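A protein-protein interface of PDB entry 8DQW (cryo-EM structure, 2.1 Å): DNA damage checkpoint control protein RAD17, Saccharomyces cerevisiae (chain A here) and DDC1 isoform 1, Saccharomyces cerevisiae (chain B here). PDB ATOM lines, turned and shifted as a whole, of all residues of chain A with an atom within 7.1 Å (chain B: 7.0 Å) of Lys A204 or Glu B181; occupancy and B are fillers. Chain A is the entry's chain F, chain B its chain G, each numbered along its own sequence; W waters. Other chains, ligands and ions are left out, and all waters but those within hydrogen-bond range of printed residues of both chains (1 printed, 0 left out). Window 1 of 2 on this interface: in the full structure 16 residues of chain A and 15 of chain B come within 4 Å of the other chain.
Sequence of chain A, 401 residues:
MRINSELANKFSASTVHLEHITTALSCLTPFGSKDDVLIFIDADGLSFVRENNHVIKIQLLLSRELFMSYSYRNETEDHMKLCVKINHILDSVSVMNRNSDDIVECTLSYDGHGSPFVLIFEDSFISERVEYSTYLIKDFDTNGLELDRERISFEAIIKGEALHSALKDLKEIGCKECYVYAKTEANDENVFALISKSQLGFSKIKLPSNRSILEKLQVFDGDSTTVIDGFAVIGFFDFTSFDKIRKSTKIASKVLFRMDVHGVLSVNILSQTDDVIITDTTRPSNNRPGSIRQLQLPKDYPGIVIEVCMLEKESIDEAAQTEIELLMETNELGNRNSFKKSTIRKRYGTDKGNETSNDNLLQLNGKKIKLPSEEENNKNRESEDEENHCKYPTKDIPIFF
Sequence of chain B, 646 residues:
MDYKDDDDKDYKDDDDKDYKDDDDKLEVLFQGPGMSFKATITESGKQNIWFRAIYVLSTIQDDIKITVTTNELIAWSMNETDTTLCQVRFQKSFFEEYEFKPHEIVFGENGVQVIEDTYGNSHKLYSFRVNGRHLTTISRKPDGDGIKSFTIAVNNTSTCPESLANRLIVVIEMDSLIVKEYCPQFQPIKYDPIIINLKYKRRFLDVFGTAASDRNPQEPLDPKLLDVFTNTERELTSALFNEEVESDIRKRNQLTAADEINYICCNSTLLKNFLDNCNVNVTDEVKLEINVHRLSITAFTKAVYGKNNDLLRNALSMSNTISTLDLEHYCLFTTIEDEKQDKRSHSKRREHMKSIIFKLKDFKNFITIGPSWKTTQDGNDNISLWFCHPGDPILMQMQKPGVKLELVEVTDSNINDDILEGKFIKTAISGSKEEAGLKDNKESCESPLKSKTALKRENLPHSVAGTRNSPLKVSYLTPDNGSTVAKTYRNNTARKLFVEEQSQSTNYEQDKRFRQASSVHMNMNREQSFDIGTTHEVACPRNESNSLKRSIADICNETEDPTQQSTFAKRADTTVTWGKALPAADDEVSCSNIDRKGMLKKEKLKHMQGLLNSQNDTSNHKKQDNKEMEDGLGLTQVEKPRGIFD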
ATOM      1  N   ASP A 169      31.718 -21.626  12.012  1.00  0.00           N
ATOM      2  CA  ASP A 169      32.498 -21.890  13.217  1.00  0.00           C
ATOM      3  C   ASP A 169      32.462 -23.369  13.580  1.00  0.00           C
ATOM      4  O   ASP A 169      33.492 -23.953  13.936  1.00  0.00           O
ATOM      5  CB  ASP A 169      31.979 -21.046  14.380  1.00  0.00           C
ATOM      6  CG  ASP A 169      32.917 -21.060  15.573  1.00  0.00           C
ATOM      7  OD1 ASP A 169      33.262 -22.162  16.049  1.00  0.00           O
ATOM      8  OD2 ASP A 169      33.317 -19.972  16.033  1.00  0.00           O
ATOM      9  N   LEU A 170      31.285 -23.990  13.498  1.00  0.00           N
ATOM     10  CA  LEU A 170      31.190 -25.413  13.808  1.00  0.00           C
ATOM     11  C   LEU A 170      32.029 -26.240  12.843  1.00  0.00           C
ATOM     12  O   LEU A 170      32.702 -27.194  13.252  1.00  0.00           O
ATOM     13  CB  LEU A 170      29.731 -25.866  13.771  1.00  0.00           C
ATOM     14  CG  LEU A 170      28.812 -25.308  14.860  1.00  0.00           C
ATOM     15  CD1 LEU A 170      27.451 -25.981  14.794  1.00  0.00           C
ATOM     16  CD2 LEU A 170      29.429 -25.470  16.241  1.00  0.00           C
ATOM     17  N   ILE A 173      35.951 -26.104  13.556  1.00  0.00           N
ATOM     18  CA  ILE A 173      36.459 -26.795  14.737  1.00  0.00           C
ATOM     19  C   ILE A 173      36.314 -28.309  14.616  1.00  0.00           C
ATOM     20  O   ILE A 173      36.559 -29.029  15.588  1.00  0.00           O
ATOM     21  CB  ILE A 173      35.777 -26.284  16.017  1.00  0.00           C
ATOM     22  CG1 ILE A 173      34.284 -26.631  16.025  1.00  0.00           C
ATOM     23  CG2 ILE A 173      35.972 -24.780  16.152  1.00  0.00           C
ATOM     24  CD1 ILE A 173      33.616 -26.391  17.361  1.00  0.00           C
ATOM     25  N   TYR A 181      19.520 -26.477  21.107  1.00  0.00           N
ATOM     26  CA  TYR A 181      18.880 -26.244  22.395  1.00  0.00           C
ATOM     27  C   TYR A 181      17.984 -25.019  22.285  1.00  0.00           C
ATOM     28  O   TYR A 181      18.446 -23.943  21.889  1.00  0.00           O
ATOM     29  CB  TYR A 181      19.936 -26.044  23.488  1.00  0.00           C
ATOM     30  CG  TYR A 181      19.385 -25.852  24.884  1.00  0.00           C
ATOM     31  CD1 TYR A 181      18.855 -24.632  25.286  1.00  0.00           C
ATOM     32  CD2 TYR A 181      19.406 -26.888  25.806  1.00  0.00           C
ATOM     33  CE1 TYR A 181      18.358 -24.454  26.563  1.00  0.00           C
ATOM     34  CE2 TYR A 181      18.911 -26.721  27.083  1.00  0.00           C
ATOM     35  CZ  TYR A 181      18.389 -25.503  27.457  1.00  0.00           C
ATOM     36  OH  TYR A 181      17.894 -25.336  28.730  1.00  0.00           O
ATOM     37  N   VAL A 191      16.301 -18.489  24.599  1.00  0.00           N
ATOM     38  CA  VAL A 191      17.637 -19.069  24.550  1.00  0.00           C
ATOM     39  C   VAL A 191      17.685 -20.113  23.445  1.00  0.00           C
ATOM     40  O   VAL A 191      17.153 -21.218  23.597  1.00  0.00           O
ATOM     41  CB  VAL A 191      18.027 -19.684  25.907  1.00  0.00           C
ATOM     42  CG1 VAL A 191      19.296 -20.514  25.774  1.00  0.00           C
ATOM     43  CG2 VAL A 191      18.203 -18.594  26.955  1.00  0.00           C
ATOM     44  N   ALA A 193      20.559 -22.094  21.125  1.00  0.00           N
ATOM     45  CA  ALA A 193      21.992 -22.348  21.114  1.00  0.00           C
ATOM     46  C   ALA A 193      22.293 -23.615  20.328  1.00  0.00           C
ATOM     47  O   ALA A 193      21.448 -24.503  20.184  1.00  0.00           O
ATOM     48  CB  ALA A 193      22.547 -22.466  22.538  1.00  0.00           C
ATOM     49  N   LEU A 194      23.519 -23.681  19.813  1.00  0.00           N
ATOM     50  CA  LEU A 194      24.058 -24.880  19.183  1.00  0.00           C
ATOM     51  C   LEU A 194      25.249 -25.350  20.005  1.00  0.00           C
ATOM     52  O   LEU A 194      26.204 -24.594  20.204  1.00  0.00           O
ATOM     53  CB  LEU A 194      24.473 -24.613  17.735  1.00  0.00           C
ATOM     54  CG  LEU A 194      23.411 -24.010  16.812  1.00  0.00           C
ATOM     55  CD1 LEU A 194      24.038 -23.573  15.497  1.00  0.00           C
ATOM     56  CD2 LEU A 194      22.283 -24.998  16.566  1.00  0.00           C
ATOM     57  N   ILE A 195      25.196 -26.594  20.473  1.00  0.00           N
ATOM     58  CA  ILE A 195      26.247 -27.181  21.293  1.00  0.00           C
ATOM     59  C   ILE A 195      26.934 -28.265  20.477  1.00  0.00           C
ATOM     60  O   ILE A 195      26.278 -29.185  19.979  1.00  0.00           O
ATOM     61  CB  ILE A 195      25.683 -27.748  22.608  1.00  0.00           C
ATOM     62  CG1 ILE A 195      25.124 -26.615  23.471  1.00  0.00           C
ATOM     63  CG2 ILE A 195      26.759 -28.514  23.365  1.00  0.00           C
ATOM     64  CD1 ILE A 195      23.615 -26.568  23.511  1.00  0.00           C
ATOM     65  N   SER A 196      28.251 -28.161  20.346  1.00  0.00           N
ATOM     66  CA  SER A 196      29.027 -29.041  19.486  1.00  0.00           C
ATOM     67  C   SER A 196      29.940 -29.924  20.322  1.00  0.00           C
ATOM     68  O   SER A 196      30.601 -29.445  21.252  1.00  0.00           O
ATOM     69  CB  SER A 196      29.859 -28.232  18.489  1.00  0.00           C
ATOM     70  OG  SER A 196      30.421 -27.090  19.106  1.00  0.00           O
ATOM     71  N   PHE A 202      33.368 -30.073  24.391  1.00  0.00           N
ATOM     72  CA  PHE A 202      32.037 -29.504  24.246  1.00  0.00           C
ATOM     73  C   PHE A 202      32.150 -27.988  24.162  1.00  0.00           C
ATOM     74  O   PHE A 202      32.767 -27.359  25.028  1.00  0.00           O
ATOM     75  CB  PHE A 202      31.136 -29.907  25.414  1.00  0.00           C
ATOM     76  CG  PHE A 202      30.534 -31.275  25.268  1.00  0.00           C
ATOM     77  CD1 PHE A 202      31.221 -32.397  25.699  1.00  0.00           C
ATOM     78  CD2 PHE A 202      29.284 -31.439  24.699  1.00  0.00           C
ATOM     79  CE1 PHE A 202      30.671 -33.658  25.566  1.00  0.00           C
ATOM     80  CE2 PHE A 202      28.728 -32.697  24.563  1.00  0.00           C
ATOM     81  CZ  PHE A 202      29.422 -33.808  24.997  1.00  0.00           C
ATOM     82  N   SER A 203      31.561 -27.410  23.118  1.00  0.00           N
ATOM     83  CA  SER A 203      31.555 -25.969  22.921  1.00  0.00           C
ATOM     84  C   SER A 203      30.128 -25.514  22.651  1.00  0.00           C
ATOM     85  O   SER A 203      29.262 -26.312  22.292  1.00  0.00           O
ATOM     86  CB  SER A 203      32.470 -25.548  21.761  1.00  0.00           C
ATOM     87  OG  SER A 203      32.277 -26.378  20.631  1.00  0.00           O
ATOM     88  N   LYS A 204      29.890 -24.218  22.830  1.00  0.00           N
ATOM     89  CA  LYS A 204      28.558 -23.649  22.683  1.00  0.00           C
ATOM     90  C   LYS A 204      28.612 -22.382  21.843  1.00  0.00           C
ATOM     91  O   LYS A 204      29.555 -21.594  21.951  1.00  0.00           O
ATOM     92  CB  LYS A 204      27.944 -23.334  24.051  1.00  0.00           C
ATOM     93  CG  LYS A 204      26.732 -22.422  23.987  1.00  0.00           C
ATOM     94  CD  LYS A 204      25.856 -22.575  25.216  1.00  0.00           C
ATOM     95  CE  LYS A 204      26.426 -21.825  26.411  1.00  0.00           C
ATOM     96  NZ  LYS A 204      25.356 -21.201  27.234  1.00  0.00           N
ATOM     97  N   ILE A 205      27.595 -22.198  21.006  1.00  0.00           N
ATOM     98  CA  ILE A 205      27.361 -20.954  20.282  1.00  0.00           C
ATOM     99  C   ILE A 205      25.943 -20.510  20.611  1.00  0.00           C
ATOM    100  O   ILE A 205      24.976 -21.198  20.259  1.00  0.00           O
ATOM    101  CB  ILE A 205      27.549 -21.121  18.765  1.00  0.00           C
ATOM    102  CG1 ILE A 205      28.869 -21.838  18.465  1.00  0.00           C
ATOM    103  CG2 ILE A 205      27.508 -19.762  18.074  1.00  0.00           C
ATOM    104  CD1 ILE A 205      29.133 -22.042  16.989  1.00  0.00           C
ATOM    105  N   LYS A 206      25.821 -19.370  21.283  1.00  0.00           N
ATOM    106  CA  LYS A 206      24.544 -18.869  21.770  1.00  0.00           C
ATOM    107  C   LYS A 206      24.089 -17.706  20.899  1.00  0.00           C
ATOM    108  O   LYS A 206      24.877 -16.803  20.600  1.00  0.00           O
ATOM    109  CB  LYS A 206      24.655 -18.423  23.230  1.00  0.00           C
ATOM    110  CG  LYS A 206      23.421 -17.708  23.765  1.00  0.00           C
ATOM    111  CD  LYS A 206      22.881 -18.384  25.012  1.00  0.00           C
ATOM    112  CE  LYS A 206      21.611 -17.704  25.500  1.00  0.00           C
ATOM    113  NZ  LYS A 206      21.825 -16.264  25.807  1.00  0.00           N
ATOM    114  N   LEU A 207      22.821 -17.736  20.494  1.00  0.00           N
ATOM    115  CA  LEU A 207      22.247 -16.660  19.693  1.00  0.00           C
ATOM    116  C   LEU A 207      21.648 -15.600  20.611  1.00  0.00           C
ATOM    117  O   LEU A 207      20.919 -15.946  21.550  1.00  0.00           O
ATOM    118  CB  LEU A 207      21.175 -17.199  18.757  1.00  0.00           C
ATOM    119  CG  LEU A 207      21.614 -17.486  17.318  1.00  0.00           C
ATOM    120  CD1 LEU A 207      22.111 -16.227  16.622  1.00  0.00           C
ATOM    121  CD2 LEU A 207      22.683 -18.568  17.296  1.00  0.00           C
ATOM    122  N   ILE A 324      25.653 -30.938  28.348  1.00  0.00           N
ATOM    123  CA  ILE A 324      24.748 -29.916  27.831  1.00  0.00           C
ATOM    124  C   ILE A 324      24.089 -29.162  28.978  1.00  0.00           C
ATOM    125  O   ILE A 324      23.997 -27.929  28.959  1.00  0.00           O
ATOM    126  CB  ILE A 324      23.700 -30.555  26.899  1.00  0.00           C
ATOM    127  CG1 ILE A 324      24.368 -31.069  25.623  1.00  0.00           C
ATOM    128  CG2 ILE A 324      22.606 -29.553  26.557  1.00  0.00           C
ATOM    129  CD1 ILE A 324      23.594 -32.164  24.929  1.00  0.00           C
ATOM    130  N   LEU A 326      25.241 -28.768  32.019  1.00  0.00           N
ATOM    131  CA  LEU A 326      26.251 -27.932  32.657  1.00  0.00           C
ATOM    132  C   LEU A 326      26.535 -26.684  31.828  1.00  0.00           C
ATOM    133  O   LEU A 326      26.674 -25.585  32.375  1.00  0.00           O
ATOM    134  CB  LEU A 326      27.531 -28.735  32.876  1.00  0.00           C
ATOM    135  CG  LEU A 326      27.454 -29.789  33.983  1.00  0.00           C
ATOM    136  CD1 LEU A 326      28.405 -30.937  33.692  1.00  0.00           C
ATOM    137  CD2 LEU A 326      27.755 -29.170  35.340  1.00  0.00           C
ATOM    138  N   LEU A 327      26.625 -26.836  30.504  1.00  0.00           N
ATOM    139  CA  LEU A 327      26.876 -25.685  29.644  1.00  0.00           C
ATOM    140  C   LEU A 327      25.734 -24.679  29.722  1.00  0.00           C
ATOM    141  O   LEU A 327      25.968 -23.466  29.783  1.00  0.00           O
ATOM    142  CB  LEU A 327      27.083 -26.144  28.200  1.00  0.00           C
ATOM    143  CG  LEU A 327      28.535 -26.358  27.769  1.00  0.00           C
ATOM    144  CD1 LEU A 327      28.601 -27.176  26.488  1.00  0.00           C
ATOM    145  CD2 LEU A 327      29.245 -25.025  27.590  1.00  0.00           C
ATOM    146  N   MET A 328      24.492 -25.160  29.716  1.00  0.00           N
ATOM    147  CA  MET A 328      23.324 -24.292  29.773  1.00  0.00           C
ATOM    148  C   MET A 328      22.928 -23.920  31.197  1.00  0.00           C
ATOM    149  O   MET A 328      21.988 -23.139  31.376  1.00  0.00           O
ATOM    150  CB  MET A 328      22.137 -24.963  29.073  1.00  0.00           C
ATOM    151  CG  MET A 328      22.409 -25.399  27.638  1.00  0.00           C
ATOM    152  SD  MET A 328      23.349 -24.199  26.673  1.00  0.00           S
ATOM    153  CE  MET A 328      22.148 -22.883  26.499  1.00  0.00           C
ATOM    154  N   GLU A 329      23.612 -24.452  32.204  1.00  0.00           N
ATOM    155  CA  GLU A 329      23.304 -24.127  33.592  1.00  0.00           C
ATOM    156  C   GLU A 329      24.548 -24.255  34.464  1.00  0.00           C
ATOM    157  O   GLU A 329      25.367 -23.340  34.533  1.00  0.00           O
ATOM    158  CB  GLU A 329      22.193 -25.036  34.122  1.00  0.00           C
ATOM    159  CG  GLU A 329      21.550 -24.542  35.409  1.00  0.00           C
ATOM    160  CD  GLU A 329      20.697 -23.307  35.196  1.00  0.00           C
ATOM    161  OE1 GLU A 329      21.265 -22.201  35.077  1.00  0.00           O
ATOM    162  OE2 GLU A 329      19.455 -23.441  35.148  1.00  0.00           O
ATOM    163  N   LEU B 164      34.031 -30.013  34.881  1.00  0.00           N
ATOM    164  CA  LEU B 164      34.685 -28.767  34.502  1.00  0.00           C
ATOM    165  C   LEU B 164      36.087 -28.631  35.080  1.00  0.00           C
ATOM    166  O   LEU B 164      36.792 -27.680  34.725  1.00  0.00           O
ATOM    167  CB  LEU B 164      33.833 -27.576  34.945  1.00  0.00           C
ATOM    168  CG  LEU B 164      32.643 -27.227  34.044  1.00  0.00           C
ATOM    169  CD1 LEU B 164      31.781 -26.157  34.692  1.00  0.00           C
ATOM    170  CD2 LEU B 164      33.112 -26.775  32.667  1.00  0.00           C
ATOM    171  N   ILE B 169      38.483 -22.194  30.461  1.00  0.00           N
ATOM    172  CA  ILE B 169      37.257 -21.589  29.950  1.00  0.00           C
ATOM    173  C   ILE B 169      37.619 -20.412  29.056  1.00  0.00           C
ATOM    174  O   ILE B 169      38.381 -19.524  29.458  1.00  0.00           O
ATOM    175  CB  ILE B 169      36.348 -21.147  31.107  1.00  0.00           C
ATOM    176  CG1 ILE B 169      35.942 -22.350  31.961  1.00  0.00           C
ATOM    177  CG2 ILE B 169      35.113 -20.435  30.574  1.00  0.00           C
ATOM    178  CD1 ILE B 169      36.147 -22.133  33.444  1.00  0.00           C
ATOM    179  N   VAL B 170      37.079 -20.403  27.839  1.00  0.00           N
ATOM    180  CA  VAL B 170      37.285 -19.318  26.887  1.00  0.00           C
ATOM    181  C   VAL B 170      35.919 -18.827  26.429  1.00  0.00           C
ATOM    182  O   VAL B 170      35.107 -19.618  25.933  1.00  0.00           O
ATOM    183  CB  VAL B 170      38.133 -19.756  25.682  1.00  0.00           C
ATOM    184  CG1 VAL B 170      38.530 -18.544  24.848  1.00  0.00           C
ATOM    185  CG2 VAL B 170      39.367 -20.518  26.146  1.00  0.00           C
ATOM    186  N   VAL B 171      35.671 -17.528  26.584  1.00  0.00           N
ATOM    187  CA  VAL B 171      34.410 -16.904  26.197  1.00  0.00           C
ATOM    188  C   VAL B 171      34.721 -15.829  25.166  1.00  0.00           C
ATOM    189  O   VAL B 171      35.521 -14.922  25.430  1.00  0.00           O
ATOM    190  CB  VAL B 171      33.676 -16.302  27.407  1.00  0.00           C
ATOM    191  CG1 VAL B 171      32.352 -15.683  26.977  1.00  0.00           C
ATOM    192  CG2 VAL B 171      33.458 -17.361  28.479  1.00  0.00           C
ATOM    193  N   ILE B 172      34.092 -15.926  23.999  1.00  0.00           N
ATOM    194  CA  ILE B 172      34.289 -14.980  22.908  1.00  0.00           C
ATOM    195  C   ILE B 172      32.958 -14.296  22.636  1.00  0.00           C
ATOM    196  O   ILE B 172      31.975 -14.957  22.278  1.00  0.00           O
ATOM    197  CB  ILE B 172      34.816 -15.669  21.639  1.00  0.00           C
ATOM    198  CG1 ILE B 172      35.997 -16.588  21.973  1.00  0.00           C
ATOM    199  CG2 ILE B 172      35.228 -14.629  20.604  1.00  0.00           C
ATOM    200  CD1 ILE B 172      36.489 -17.399  20.798  1.00  0.00           C
ATOM    201  N   VAL B 179      27.680 -15.192  21.275  1.00  0.00           N
ATOM    202  CA  VAL B 179      28.622 -15.621  22.303  1.00  0.00           C
ATOM    203  C   VAL B 179      29.023 -17.061  22.018  1.00  0.00           C
ATOM    204  O   VAL B 179      28.162 -17.916  21.782  1.00  0.00           O
ATOM    205  CB  VAL B 179      28.020 -15.493  23.715  1.00  0.00           C
ATOM    206  CG1 VAL B 179      29.017 -15.968  24.765  1.00  0.00           C
ATOM    207  CG2 VAL B 179      27.597 -14.057  23.987  1.00  0.00           C
ATOM    208  N   LYS B 180      30.328 -17.324  22.035  1.00  0.00           N
ATOM    209  CA  LYS B 180      30.876 -18.662  21.865  1.00  0.00           C
ATOM    210  C   LYS B 180      31.654 -19.044  23.116  1.00  0.00           C
ATOM    211  O   LYS B 180      32.349 -18.210  23.704  1.00  0.00           O
ATOM    212  CB  LYS B 180      31.789 -18.741  20.635  1.00  0.00           C
ATOM    213  CG  LYS B 180      31.396 -17.798  19.504  1.00  0.00           C
ATOM    214  CD  LYS B 180      31.865 -18.301  18.142  1.00  0.00           C
ATOM    215  CE  LYS B 180      33.082 -17.538  17.638  1.00  0.00           C
ATOM    216  NZ  LYS B 180      33.161 -17.538  16.151  1.00  0.00           N
ATOM    217  N   GLU B 181      31.528 -20.303  23.528  1.00  0.00           N
ATOM    218  CA  GLU B 181      32.192 -20.800  24.725  1.00  0.00           C
ATOM    219  C   GLU B 181      32.953 -22.078  24.407  1.00  0.00           C
ATOM    220  O   GLU B 181      32.452 -22.948  23.689  1.00  0.00           O
ATOM    221  CB  GLU B 181      31.187 -21.064  25.852  1.00  0.00           C
ATOM    222  CG  GLU B 181      31.702 -20.678  27.228  1.00  0.00           C
ATOM    223  CD  GLU B 181      30.821 -21.187  28.352  1.00  0.00           C
ATOM    224  OE1 GLU B 181      30.406 -22.363  28.301  1.00  0.00           O
ATOM    225  OE2 GLU B 181      30.544 -20.408  29.289  1.00  0.00           O
ATOM    226  N   TYR B 182      34.168 -22.180  24.945  1.00  0.00           N
ATOM    227  CA  TYR B 182      35.003 -23.363  24.792  1.00  0.00           C
ATOM    228  C   TYR B 182      35.609 -23.720  26.143  1.00  0.00           C
ATOM    229  O   TYR B 182      35.779 -22.856  27.008  1.00  0.00           O
ATOM    230  CB  TYR B 182      36.130 -23.146  23.771  1.00  0.00           C
ATOM    231  CG  TYR B 182      35.679 -22.614  22.430  1.00  0.00           C
ATOM    232  CD1 TYR B 182      35.312 -23.478  21.406  1.00  0.00           C
ATOM    233  CD2 TYR B 182      35.637 -21.248  22.181  1.00  0.00           C
ATOM    234  CE1 TYR B 182      34.907 -22.996  20.176  1.00  0.00           C
ATOM    235  CE2 TYR B 182      35.233 -20.757  20.954  1.00  0.00           C
ATOM    236  CZ  TYR B 182      34.869 -21.636  19.955  1.00  0.00           C
ATOM    237  OH  TYR B 182      34.467 -21.153  18.733  1.00  0.00           O
ATOM    238  N   CYS B 183      35.946 -24.999  26.315  1.00  0.00           N
ATOM    239  CA  CYS B 183      36.574 -25.480  27.548  1.00  0.00           C
ATOM    240  C   CYS B 183      37.535 -26.615  27.219  1.00  0.00           C
ATOM    241  O   CYS B 183      37.313 -27.772  27.593  1.00  0.00           O
ATOM    242  CB  CYS B 183      35.517 -25.932  28.554  1.00  0.00           C
ATOM    243  SG  CYS B 183      34.227 -26.986  27.855  1.00  0.00           S
ATOM    244  N   PRO B 184      38.622 -26.317  26.510  1.00  0.00           N
ATOM    245  CA  PRO B 184      39.640 -27.348  26.270  1.00  0.00           C
ATOM    246  C   PRO B 184      40.297 -27.793  27.569  1.00  0.00           C
ATOM    247  O   PRO B 184      40.518 -26.997  28.483  1.00  0.00           O
ATOM    248  CB  PRO B 184      40.640 -26.652  25.339  1.00  0.00           C
ATOM    249  CG  PRO B 184      40.418 -25.192  25.555  1.00  0.00           C
ATOM    250  CD  PRO B 184      38.958 -25.048  25.844  1.00  0.00           C
HETATM  251  O   HOH W   1      35.486 -26.925  24.211  1.00  0.00           O
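Among the printed residues, pairs that only touch across the chains: Ser A203 with Glu B181 (3.2 Å), Ser A203 with Tyr B182 (3.5 Å), Lys A204 with Val B179 (3.9 Å), Lys A204 with Lys B180 (3.2 Å), Ile A205 with Val B179 (3.5 Å) and Leu A327 with Glu B181 (3.0 Å).
The side-chain carboxylate (OD2) of Asp A169 lies within salt-bridge range of the side-chain amino group (NZ) of Lys B180, at 2.4 Å.
The side-chain carboxylate of Asp A169 is in hydrogen-bond range of the side-chain hydroxyl of Tyr B182.
The backbone carbonyl oxygen (O) of Phe A202 sits at hydrogen-bond distance from the side-chain sulfur (SG) of Cys B183 (3.2 Å).
N of Glu B181 lies within hydrogen-bond range of O of Lys A204, at 2.8 Å.
The backbone carbonyl oxygen (O) of Val B179 is in hydrogen-bond range of the backbone NH (N) of Lys A206.
Printed residues of chain B that touch a printed residue of chain A: Val B179, Lys B180, Glu B181, Tyr B182 and Cys B183.
Hydrophobic or aromatic side chains of chain B that line the printed part of chain A: Tyr B182.
Of the 20 printed residues of chain A, 7 touch a printed residue of chain B.
Printed residues of chain A that touch a printed residue of chain B: Asp A169, Phe A202, Ser A203, Lys A204, Ile A205, Lys A206 and Leu A327.
Hydrophobic or aromatic side chains of chain A that line the printed part of chain B: Leu A327.
Along chain A the printed residues that touch a printed residue of chain B span positions 169 to 327.
Among the printed residues, Asp or Glu carboxylates within 4 Å of a Lys or Arg side-chain nitrogen of the other chain: Asp A169 with Lys B180 (2.4 Å).
Of chain B, only Val B179 (3.9 Å), Lys B180 (3.2 Å) and Glu B181 (2.8 Å) come within 4 Å of Lys A204.
Printed residues of chain A within 4 Å of Glu B181: Ser A203, Lys A204 and Leu A327.
Printed residues of chain B within 4 Å of Phe A202: Cys B183.
Of the printed residues of chain A, Val B179 touches Lys A204 (3.9 Å), Ile A205 (3.5 Å) and Lys A206 (2.8 Å).
Of the printed residues of chain B, Ser A203 touches Glu B181 and Tyr B182.
Ile B169 touches none of the printed residues of chain A.
The nearest residue of chain B that does not touch Lys A204 is Tyr B182 (5.2 Å).
Water W1 bridges the backbone carbonyl oxygen of Phe A202 (2.9 Å) and the backbone NH of Cys B183 (2.9 Å).
O of Tyr B182 lies within hydrogen-bond range of N of Val B170 (2.9 Å).
The side-chain sulfur of Met A328 sits close to the side-chain amino group of Lys A204, 3.7 Å away.
O of Leu A194 is in hydrogen-bond range of N of Ile A205.
The backbone NH (N) of Ile B172 is in hydrogen-bond range of the backbone carbonyl oxygen (O) of Lys B180 (2.9 Å).
The side-chain hydroxyl (OG) of Ser A203 sits at hydrogen-bond distance from the side-chain hydroxyl (OG) of Ser A196 (2.5 Å).
NZ of Lys A204 sits at hydrogen-bond distance from O of Leu A327, at 3.5 Å.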
